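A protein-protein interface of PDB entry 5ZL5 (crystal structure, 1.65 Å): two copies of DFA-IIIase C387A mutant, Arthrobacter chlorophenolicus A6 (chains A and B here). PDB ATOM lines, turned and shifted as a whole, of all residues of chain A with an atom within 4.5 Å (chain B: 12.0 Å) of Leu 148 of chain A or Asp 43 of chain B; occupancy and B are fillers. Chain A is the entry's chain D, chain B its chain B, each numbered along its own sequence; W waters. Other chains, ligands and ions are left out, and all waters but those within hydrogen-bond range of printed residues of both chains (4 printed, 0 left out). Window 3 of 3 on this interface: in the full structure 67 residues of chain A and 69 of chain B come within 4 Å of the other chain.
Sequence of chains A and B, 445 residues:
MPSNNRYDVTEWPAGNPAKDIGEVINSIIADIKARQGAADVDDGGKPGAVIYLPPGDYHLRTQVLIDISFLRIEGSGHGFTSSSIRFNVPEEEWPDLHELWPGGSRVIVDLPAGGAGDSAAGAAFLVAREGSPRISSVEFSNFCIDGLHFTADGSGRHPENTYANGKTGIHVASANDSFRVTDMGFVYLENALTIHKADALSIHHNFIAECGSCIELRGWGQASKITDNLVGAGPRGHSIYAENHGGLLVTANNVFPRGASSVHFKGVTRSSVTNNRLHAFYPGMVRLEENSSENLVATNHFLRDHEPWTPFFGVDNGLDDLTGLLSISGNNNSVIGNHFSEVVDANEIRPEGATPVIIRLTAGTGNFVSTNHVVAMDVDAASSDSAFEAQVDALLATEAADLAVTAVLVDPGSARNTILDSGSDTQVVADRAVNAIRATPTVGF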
ATOM      1  N   HIS A  59     -17.989   6.374  20.681  1.00  0.00           N
ATOM      2  CA  HIS A  59     -17.087   5.482  19.980  1.00  0.00           C
ATOM      3  C   HIS A  59     -17.910   4.569  19.108  1.00  0.00           C
ATOM      4  O   HIS A  59     -18.935   4.017  19.552  1.00  0.00           O
ATOM      5  CB  HIS A  59     -16.246   4.659  20.969  1.00  0.00           C
ATOM      6  CG  HIS A  59     -15.236   5.485  21.715  1.00  0.00           C
ATOM      7  ND1 HIS A  59     -13.920   5.569  21.328  1.00  0.00           N
ATOM      8  CD2 HIS A  59     -15.360   6.291  22.794  1.00  0.00           C
ATOM      9  CE1 HIS A  59     -13.266   6.372  22.151  1.00  0.00           C
ATOM     10  NE2 HIS A  59     -14.121   6.825  23.050  1.00  0.00           N
ATOM     11  N   PHE A  87      -1.620  17.820  17.121  1.00  0.00           N
ATOM     12  CA  PHE A  87      -0.596  16.767  17.071  1.00  0.00           C
ATOM     13  C   PHE A  87       0.797  17.269  16.733  1.00  0.00           C
ATOM     14  O   PHE A  87       1.757  16.545  16.966  1.00  0.00           O
ATOM     15  CB  PHE A  87      -0.985  15.650  16.112  1.00  0.00           C
ATOM     16  CG  PHE A  87      -2.116  14.792  16.610  1.00  0.00           C
ATOM     17  CD1 PHE A  87      -2.076  14.209  17.880  1.00  0.00           C
ATOM     18  CD2 PHE A  87      -3.207  14.525  15.801  1.00  0.00           C
ATOM     19  CE1 PHE A  87      -3.102  13.411  18.345  1.00  0.00           C
ATOM     20  CE2 PHE A  87      -4.250  13.735  16.263  1.00  0.00           C
ATOM     21  CZ  PHE A  87      -4.204  13.176  17.535  1.00  0.00           C
ATOM     22  N   TRP A 101      -9.483  17.448  21.640  1.00  0.00           N
ATOM     23  CA  TRP A 101     -10.184  16.631  20.651  1.00  0.00           C
ATOM     24  C   TRP A 101     -11.315  17.401  20.003  1.00  0.00           C
ATOM     25  O   TRP A 101     -11.816  18.345  20.588  1.00  0.00           O
ATOM     26  CB  TRP A 101     -10.774  15.412  21.331  1.00  0.00           C
ATOM     27  CG  TRP A 101      -9.737  14.455  21.896  1.00  0.00           C
ATOM     28  CD1 TRP A 101      -9.460  14.229  23.215  1.00  0.00           C
ATOM     29  CD2 TRP A 101      -8.878  13.598  21.152  1.00  0.00           C
ATOM     30  NE1 TRP A 101      -8.471  13.290  23.335  1.00  0.00           N
ATOM     31  CE2 TRP A 101      -8.099  12.875  22.084  1.00  0.00           C
ATOM     32  CE3 TRP A 101      -8.681  13.364  19.797  1.00  0.00           C
ATOM     33  CZ2 TRP A 101      -7.143  11.920  21.683  1.00  0.00           C
ATOM     34  CZ3 TRP A 101      -7.717  12.415  19.402  1.00  0.00           C
ATOM     35  CH2 TRP A 101      -6.976  11.707  20.345  1.00  0.00           C
ATOM     36  N   ARG A 106     -20.258  13.789  18.171  1.00  0.00           N
ATOM     37  CA  ARG A 106     -19.030  13.193  17.663  1.00  0.00           C
ATOM     38  C   ARG A 106     -19.013  11.669  17.621  1.00  0.00           C
ATOM     39  O   ARG A 106     -19.136  11.005  18.652  1.00  0.00           O
ATOM     40  CB  ARG A 106     -17.862  13.668  18.516  1.00  0.00           C
ATOM     41  CG  ARG A 106     -16.498  13.109  18.128  1.00  0.00           C
ATOM     42  CD  ARG A 106     -15.456  13.908  18.878  1.00  0.00           C
ATOM     43  NE  ARG A 106     -14.091  13.374  18.758  1.00  0.00           N
ATOM     44  CZ  ARG A 106     -13.328  12.945  19.767  1.00  0.00           C
ATOM     45  NH1 ARG A 106     -13.771  12.916  21.007  1.00  0.00           N
ATOM     46  NH2 ARG A 106     -12.099  12.504  19.514  1.00  0.00           N
ATOM     47  N   ILE A 108     -16.565   8.796  16.908  1.00  0.00           N
ATOM     48  CA  ILE A 108     -15.141   8.404  16.858  1.00  0.00           C
ATOM     49  C   ILE A 108     -15.053   7.049  16.151  1.00  0.00           C
ATOM     50  O   ILE A 108     -15.613   6.068  16.636  1.00  0.00           O
ATOM     51  CB  ILE A 108     -14.541   8.273  18.261  1.00  0.00           C
ATOM     52  CG1 ILE A 108     -14.633   9.603  19.017  1.00  0.00           C
ATOM     53  CG2 ILE A 108     -13.081   7.790  18.197  1.00  0.00           C
ATOM     54  CD1 ILE A 108     -14.442   9.465  20.515  1.00  0.00           C
ATOM     55  N   ASP A 110     -13.574   3.913  15.488  1.00  0.00           N
ATOM     56  CA  ASP A 110     -12.604   2.935  16.041  1.00  0.00           C
ATOM     57  C   ASP A 110     -12.703   1.612  15.289  1.00  0.00           C
ATOM     58  O   ASP A 110     -12.800   0.559  15.910  1.00  0.00           O
ATOM     59  CB  ASP A 110     -12.865   2.666  17.523  1.00  0.00           C
ATOM     60  CG  ASP A 110     -12.561   3.845  18.428  1.00  0.00           C
ATOM     61  OD1 ASP A 110     -11.549   4.555  18.228  1.00  0.00           O
ATOM     62  OD2 ASP A 110     -13.324   4.027  19.406  1.00  0.00           O
ATOM     63  N   ASP A 146     -14.905  11.574  13.260  1.00  0.00           N
ATOM     64  CA  ASP A 146     -13.504  11.787  13.629  1.00  0.00           C
ATOM     65  C   ASP A 146     -12.773  10.450  13.572  1.00  0.00           C
ATOM     66  O   ASP A 146     -13.141   9.519  14.282  1.00  0.00           O
ATOM     67  CB  ASP A 146     -13.505  12.380  15.030  1.00  0.00           C
ATOM     68  CG  ASP A 146     -12.116  12.680  15.581  1.00  0.00           C
ATOM     69  OD1 ASP A 146     -11.079  12.517  14.877  1.00  0.00           O
ATOM     70  OD2 ASP A 146     -12.114  13.107  16.772  1.00  0.00           O
ATOM     71  N   GLY A 147     -11.731  10.366  12.746  1.00  0.00           N
ATOM     72  CA  GLY A 147     -10.889   9.153  12.671  1.00  0.00           C
ATOM     73  C   GLY A 147      -9.719   9.174  13.638  1.00  0.00           C
ATOM     74  O   GLY A 147      -8.831   8.323  13.541  1.00  0.00           O
ATOM     75  N   LEU A 148      -9.697  10.174  14.527  1.00  0.00           N
ATOM     76  CA  LEU A 148      -8.828  10.200  15.711  1.00  0.00           C
ATOM     77  C   LEU A 148      -7.334  10.426  15.462  1.00  0.00           C
ATOM     78  O   LEU A 148      -6.793  11.448  15.911  1.00  0.00           O
ATOM     79  CB  LEU A 148      -9.071   8.937  16.565  1.00  0.00           C
ATOM     80  CG  LEU A 148      -8.997   9.121  18.067  1.00  0.00           C
ATOM     81  CD1 LEU A 148     -10.083  10.056  18.563  1.00  0.00           C
ATOM     82  CD2 LEU A 148      -9.115   7.754  18.745  1.00  0.00           C
ATOM     83  N   HIS A 149      -6.687   9.482  14.775  1.00  0.00           N
ATOM     84  CA  HIS A 149      -5.238   9.514  14.505  1.00  0.00           C
ATOM     85  C   HIS A 149      -4.916   9.153  13.059  1.00  0.00           C
ATOM     86  O   HIS A 149      -5.633   8.362  12.431  1.00  0.00           O
ATOM     87  CB  HIS A 149      -4.500   8.487  15.370  1.00  0.00           C
ATOM     88  CG  HIS A 149      -4.595   8.731  16.843  1.00  0.00           C
ATOM     89  ND1 HIS A 149      -3.809   9.655  17.499  1.00  0.00           N
ATOM     90  CD2 HIS A 149      -5.351   8.141  17.795  1.00  0.00           C
ATOM     91  CE1 HIS A 149      -4.086   9.634  18.790  1.00  0.00           C
ATOM     92  NE2 HIS A 149      -5.013   8.719  18.999  1.00  0.00           N
ATOM     93  N   TYR A 188      -9.701  13.978  10.316  1.00  0.00           N
ATOM     94  CA  TYR A 188      -8.735  12.892  10.562  1.00  0.00           C
ATOM     95  C   TYR A 188      -9.214  11.521  10.028  1.00  0.00           C
ATOM     96  O   TYR A 188      -8.946  10.486  10.608  1.00  0.00           O
ATOM     97  CB  TYR A 188      -8.273  12.904  12.046  1.00  0.00           C
ATOM     98  CG  TYR A 188      -6.898  13.515  12.155  1.00  0.00           C
ATOM     99  CD1 TYR A 188      -6.667  14.818  11.716  1.00  0.00           C
ATOM    100  CD2 TYR A 188      -5.808  12.779  12.636  1.00  0.00           C
ATOM    101  CE1 TYR A 188      -5.401  15.373  11.717  1.00  0.00           C
ATOM    102  CE2 TYR A 188      -4.528  13.343  12.664  1.00  0.00           C
ATOM    103  CZ  TYR A 188      -4.328  14.631  12.191  1.00  0.00           C
ATOM    104  OH  TYR A 188      -3.075  15.200  12.204  1.00  0.00           O
ATOM    105  N   GLN B  36     -17.944  19.049  32.102  1.00  0.00           N
ATOM    106  CA  GLN B  36     -16.912  18.778  31.106  1.00  0.00           C
ATOM    107  C   GLN B  36     -15.567  19.419  31.496  1.00  0.00           C
ATOM    108  O   GLN B  36     -15.080  20.338  30.835  1.00  0.00           O
ATOM    109  CB  GLN B  36     -17.379  19.293  29.729  1.00  0.00           C
ATOM    110  CG  GLN B  36     -18.657  18.620  29.252  1.00  0.00           C
ATOM    111  CD  GLN B  36     -19.087  19.017  27.846  1.00  0.00           C
ATOM    112  OE1 GLN B  36     -18.336  19.638  27.099  1.00  0.00           O
ATOM    113  NE2 GLN B  36     -20.312  18.632  27.476  1.00  0.00           N
ATOM    114  N   GLY B  37     -14.979  18.926  32.584  1.00  0.00           N
ATOM    115  CA  GLY B  37     -13.721  19.463  33.122  1.00  0.00           C
ATOM    116  C   GLY B  37     -12.436  18.826  32.602  1.00  0.00           C
ATOM    117  O   GLY B  37     -11.373  19.459  32.650  1.00  0.00           O
ATOM    118  N   ALA B  38     -12.523  17.585  32.115  1.00  0.00           N
ATOM    119  CA  ALA B  38     -11.360  16.826  31.664  1.00  0.00           C
ATOM    120  C   ALA B  38     -11.297  16.791  30.133  1.00  0.00           C
ATOM    121  O   ALA B  38     -12.283  16.450  29.470  1.00  0.00           O
ATOM    122  CB  ALA B  38     -11.410  15.416  32.230  1.00  0.00           C
ATOM    123  N   ALA B  39     -10.137  17.141  29.585  1.00  0.00           N
ATOM    124  CA  ALA B  39      -9.934  17.204  28.129  1.00  0.00           C
ATOM    125  C   ALA B  39      -9.526  15.882  27.448  1.00  0.00           C
ATOM    126  O   ALA B  39      -9.564  15.802  26.216  1.00  0.00           O
ATOM    127  CB  ALA B  39      -8.912  18.286  27.796  1.00  0.00           C
ATOM    128  N   ASP B  40      -9.137  14.857  28.206  1.00  0.00           N
ATOM    129  CA  ASP B  40      -8.587  13.627  27.592  1.00  0.00           C
ATOM    130  C   ASP B  40      -8.966  12.371  28.376  1.00  0.00           C
ATOM    131  O   ASP B  40      -8.123  11.684  28.958  1.00  0.00           O
ATOM    132  CB  ASP B  40      -7.057  13.759  27.428  1.00  0.00           C
ATOM    133  CG  ASP B  40      -6.453  12.679  26.531  1.00  0.00           C
ATOM    134  OD1 ASP B  40      -7.143  12.141  25.643  1.00  0.00           O
ATOM    135  OD2 ASP B  40      -5.263  12.370  26.712  1.00  0.00           O
ATOM    136  N   VAL B  41     -10.267  12.098  28.377  1.00  0.00           N
ATOM    137  CA  VAL B  41     -10.840  10.905  28.979  1.00  0.00           C
ATOM    138  C   VAL B  41     -11.470  10.134  27.838  1.00  0.00           C
ATOM    139  O   VAL B  41     -12.339  10.671  27.154  1.00  0.00           O
ATOM    140  CB  VAL B  41     -11.923  11.259  30.015  1.00  0.00           C
ATOM    141  CG1 VAL B  41     -12.477   9.999  30.675  1.00  0.00           C
ATOM    142  CG2 VAL B  41     -11.348  12.192  31.073  1.00  0.00           C
ATOM    143  N   ASP B  42     -11.004   8.900  27.629  1.00  0.00           N
ATOM    144  CA  ASP B  42     -11.455   8.021  26.534  1.00  0.00           C
ATOM    145  C   ASP B  42     -11.526   8.763  25.199  1.00  0.00           C
ATOM    146  O   ASP B  42     -12.555   8.735  24.492  1.00  0.00           O
ATOM    147  CB  ASP B  42     -12.805   7.381  26.866  1.00  0.00           C
ATOM    148  CG  ASP B  42     -12.741   6.481  28.076  1.00  0.00           C
ATOM    149  OD1 ASP B  42     -11.810   5.644  28.154  1.00  0.00           O
ATOM    150  OD2 ASP B  42     -13.634   6.601  28.941  1.00  0.00           O
ATOM    151  N   ASP B  43     -10.432   9.450  24.885  1.00  0.00           N
ATOM    152  CA  ASP B  43     -10.294  10.214  23.619  1.00  0.00           C
ATOM    153  C   ASP B  43     -11.319  11.331  23.422  1.00  0.00           C
ATOM    154  O   ASP B  43     -11.675  11.653  22.293  1.00  0.00           O
ATOM    155  CB  ASP B  43     -10.345   9.283  22.410  1.00  0.00           C
ATOM    156  CG  ASP B  43      -9.335   8.168  22.490  1.00  0.00           C
ATOM    157  OD1 ASP B  43      -8.202   8.436  22.902  1.00  0.00           O
ATOM    158  OD2 ASP B  43      -9.674   7.031  22.137  1.00  0.00           O
ATOM    159  N   GLY B  44     -11.754  11.937  24.513  1.00  0.00           N
ATOM    160  CA  GLY B  44     -12.760  13.010  24.467  1.00  0.00           C
ATOM    161  C   GLY B  44     -12.814  13.715  25.795  1.00  0.00           C
ATOM    162  O   GLY B  44     -11.827  13.700  26.568  1.00  0.00           O
ATOM    163  N   GLY B  45     -13.960  14.332  26.068  1.00  0.00           N
ATOM    164  CA  GLY B  45     -14.259  14.871  27.390  1.00  0.00           C
ATOM    165  C   GLY B  45     -14.899  16.255  27.400  1.00  0.00           C
ATOM    166  O   GLY B  45     -15.594  16.599  28.369  1.00  0.00           O
ATOM    167  N   LYS B  46     -14.675  17.039  26.338  1.00  0.00           N
ATOM    168  CA  LYS B  46     -15.269  18.387  26.209  1.00  0.00           C
ATOM    169  C   LYS B  46     -15.997  18.534  24.873  1.00  0.00           C
ATOM    170  O   LYS B  46     -15.650  19.386  24.059  1.00  0.00           O
ATOM    171  CB  LYS B  46     -14.207  19.475  26.358  1.00  0.00           C
ATOM    172  CG  LYS B  46     -13.545  19.510  27.726  1.00  0.00           C
ATOM    173  CD  LYS B  46     -12.621  20.711  27.860  1.00  0.00           C
ATOM    174  CE  LYS B  46     -12.034  20.888  29.263  1.00  0.00           C
ATOM    175  NZ  LYS B  46     -11.365  22.233  29.361  1.00  0.00           N
ATOM    176  N   PRO B  47     -17.034  17.718  24.660  1.00  0.00           N
ATOM    177  CA  PRO B  47     -17.755  17.766  23.371  1.00  0.00           C
ATOM    178  C   PRO B  47     -18.685  18.976  23.191  1.00  0.00           C
ATOM    179  O   PRO B  47     -19.178  19.202  22.079  1.00  0.00           O
ATOM    180  CB  PRO B  47     -18.565  16.470  23.410  1.00  0.00           C
ATOM    181  CG  PRO B  47     -18.873  16.279  24.863  1.00  0.00           C
ATOM    182  CD  PRO B  47     -17.614  16.701  25.560  1.00  0.00           C
ATOM    183  N   GLY B  48     -18.949  19.740  24.247  1.00  0.00           N
ATOM    184  CA  GLY B  48     -19.820  20.906  24.138  1.00  0.00           C
ATOM    185  C   GLY B  48     -21.256  20.521  24.374  1.00  0.00           C
ATOM    186  O   GLY B  48     -21.535  19.544  25.076  1.00  0.00           O
ATOM    187  N   PHE B  70     -17.493  24.259  20.580  1.00  0.00           N
ATOM    188  CA  PHE B  70     -18.548  23.297  20.230  1.00  0.00           C
ATOM    189  C   PHE B  70     -19.883  23.567  20.930  1.00  0.00           C
ATOM    190  O   PHE B  70     -20.647  22.619  21.213  1.00  0.00           O
ATOM    191  CB  PHE B  70     -18.111  21.841  20.488  1.00  0.00           C
ATOM    192  CG  PHE B  70     -16.655  21.560  20.225  1.00  0.00           C
ATOM    193  CD1 PHE B  70     -16.065  21.834  18.985  1.00  0.00           C
ATOM    194  CD2 PHE B  70     -15.866  21.015  21.216  1.00  0.00           C
ATOM    195  CE1 PHE B  70     -14.716  21.572  18.753  1.00  0.00           C
ATOM    196  CE2 PHE B  70     -14.523  20.735  20.980  1.00  0.00           C
ATOM    197  CZ  PHE B  70     -13.949  20.999  19.753  1.00  0.00           C
HETATM  198  O   HOH W   1      -5.888   8.116  21.466  1.00  0.00           O
HETATM  199  O   HOH W   2     -12.867  18.442  23.220  1.00  0.00           O
HETATM  200  O   HOH W   3     -10.490  17.656  24.553  1.00  0.00           O
HETATM  201  O   HOH W   4     -10.529   5.134  20.550  1.00  0.00           O
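OD1 of Asp 40 of chain B sits at hydrogen-bond distance from NE1 of Trp 101 of chain A (2.9 Å). O of Asp 42 of chain B lies within hydrogen-bond range of NE2 of His 59 of chain A (2.9 Å). The guanidinium group (NH1) of Arg 106 of chain A is in hydrogen-bond range of the backbone carbonyl oxygen (O) of Asp 43 of chain B (2.8 Å).
A ring nitrogen (ND1) of His 59 of chain A is in hydrogen-bond range of the side-chain carboxylate of Asp 110 of chain A (2.5 Å). The side-chain carboxylate of Asp 146 of chain A lies within salt-bridge range of the guanidinium group of Arg 106 of chain A (2.8 Å). The backbone NH of Leu 148 of chain A is in hydrogen-bond range of the side-chain carboxylate of Asp 146 of chain A.
CE1 of His 59 of chain A touches OD2 of Asp 43 of chain B, at 3.7 Å. Trp 101 of chain A touches Ala 39 of chain B. Trp 101 of chain A touches Asp 43 of chain B. CD1 of Trp 101 of chain A touches N of Gly 44 of chain B, at 3.5 Å. Phe 70 of chain B touches Trp 101 of chain A. NH1 of Arg 106 of chain A touches CA of Gly 44 of chain B, at 3.6 Å. CD1 of Ile 108 of chain A touches O of Asp 43 of chain B (3.95 Å). Leu 148 of chain A touches Asp 43 of chain B.
Of chain B, only Ala 39, Asp 40, Asp 43, Gly 44 and Phe 70 come within 4 Å of Trp 101 of chain A. Of the printed residues of chain B, Arg 106 of chain A touches Asp 43 and Gly 44. Of chain B, only Asp 43 (3.95 Å) comes within 4 Å of Ile 108 of chain A. Leu 148 of chain A touches just one residue of chain B: Asp 43 (3.5 Å). Val 41 of chain B touches none of the printed residues of chain A. Of the printed residues of chain A, Asp 42 of chain B touches His 59 (2.9 Å). Asp 43 of chain B touches just these residues of chain A: His 59 (3.7 Å), Trp 101 (3.4 Å), Arg 106 (2.8 Å), Ile 108 (3.95 Å) and Leu 148 (3.5 Å). Printed residues of chain A within 4 Å of Gly 44 of chain B: Trp 101 and Arg 106. Gly 45 of chain B touches none of the printed residues of chain A. Printed residues of chain A within 4 Å of Phe 70 of chain B: Trp 101. The nearest residue of chain B that does not touch Leu 148 of chain A is Gly 44 of chain B (6.5 Å). The nearest printed residue of chain A that does not touch Asp 43 of chain B is Asp 110 of chain A (5.0 Å).
Hydrophobic or aromatic side chains of chain A that line the printed part of chain B: His 59, Trp 101, Ile 108 and Leu 148. Along chain A the printed residues that touch a printed residue of chain B span positions 59 to 148. Printed residues of chain B that touch a printed residue of chain A: Ala 39, Asp 40, Asp 42, Asp 43, Gly 44 and Phe 70. Among the printed residues, no Asp or Glu carboxylate lies within 4 Å of a Lys or Arg side-chain nitrogen of the other chain.
No position is printed for both chains.
Water W4 bridges the side-chain carboxylate of Asp 110 of chain A (2.6 Å) and the side-chain carboxylate of Asp 43 of chain B (2.6 Å). Water W3 lies within hydrogen-bond range of the backbone carbonyl oxygen of Ala 39 of chain B (2.7 Å) and the backbone NH of Trp 101 of chain A (3.1 Å). Water W1 lies within hydrogen-bond range of a ring nitrogen (NE2) of His 149 of chain A (2.7 Å) and the side-chain carboxylate (OD1) of Asp 43 of chain B (2.7 Å). Water W2 bridges O of Trp 101 of chain A (2.8 Å) and O of Lys 46 of chain B (3.1 Å).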
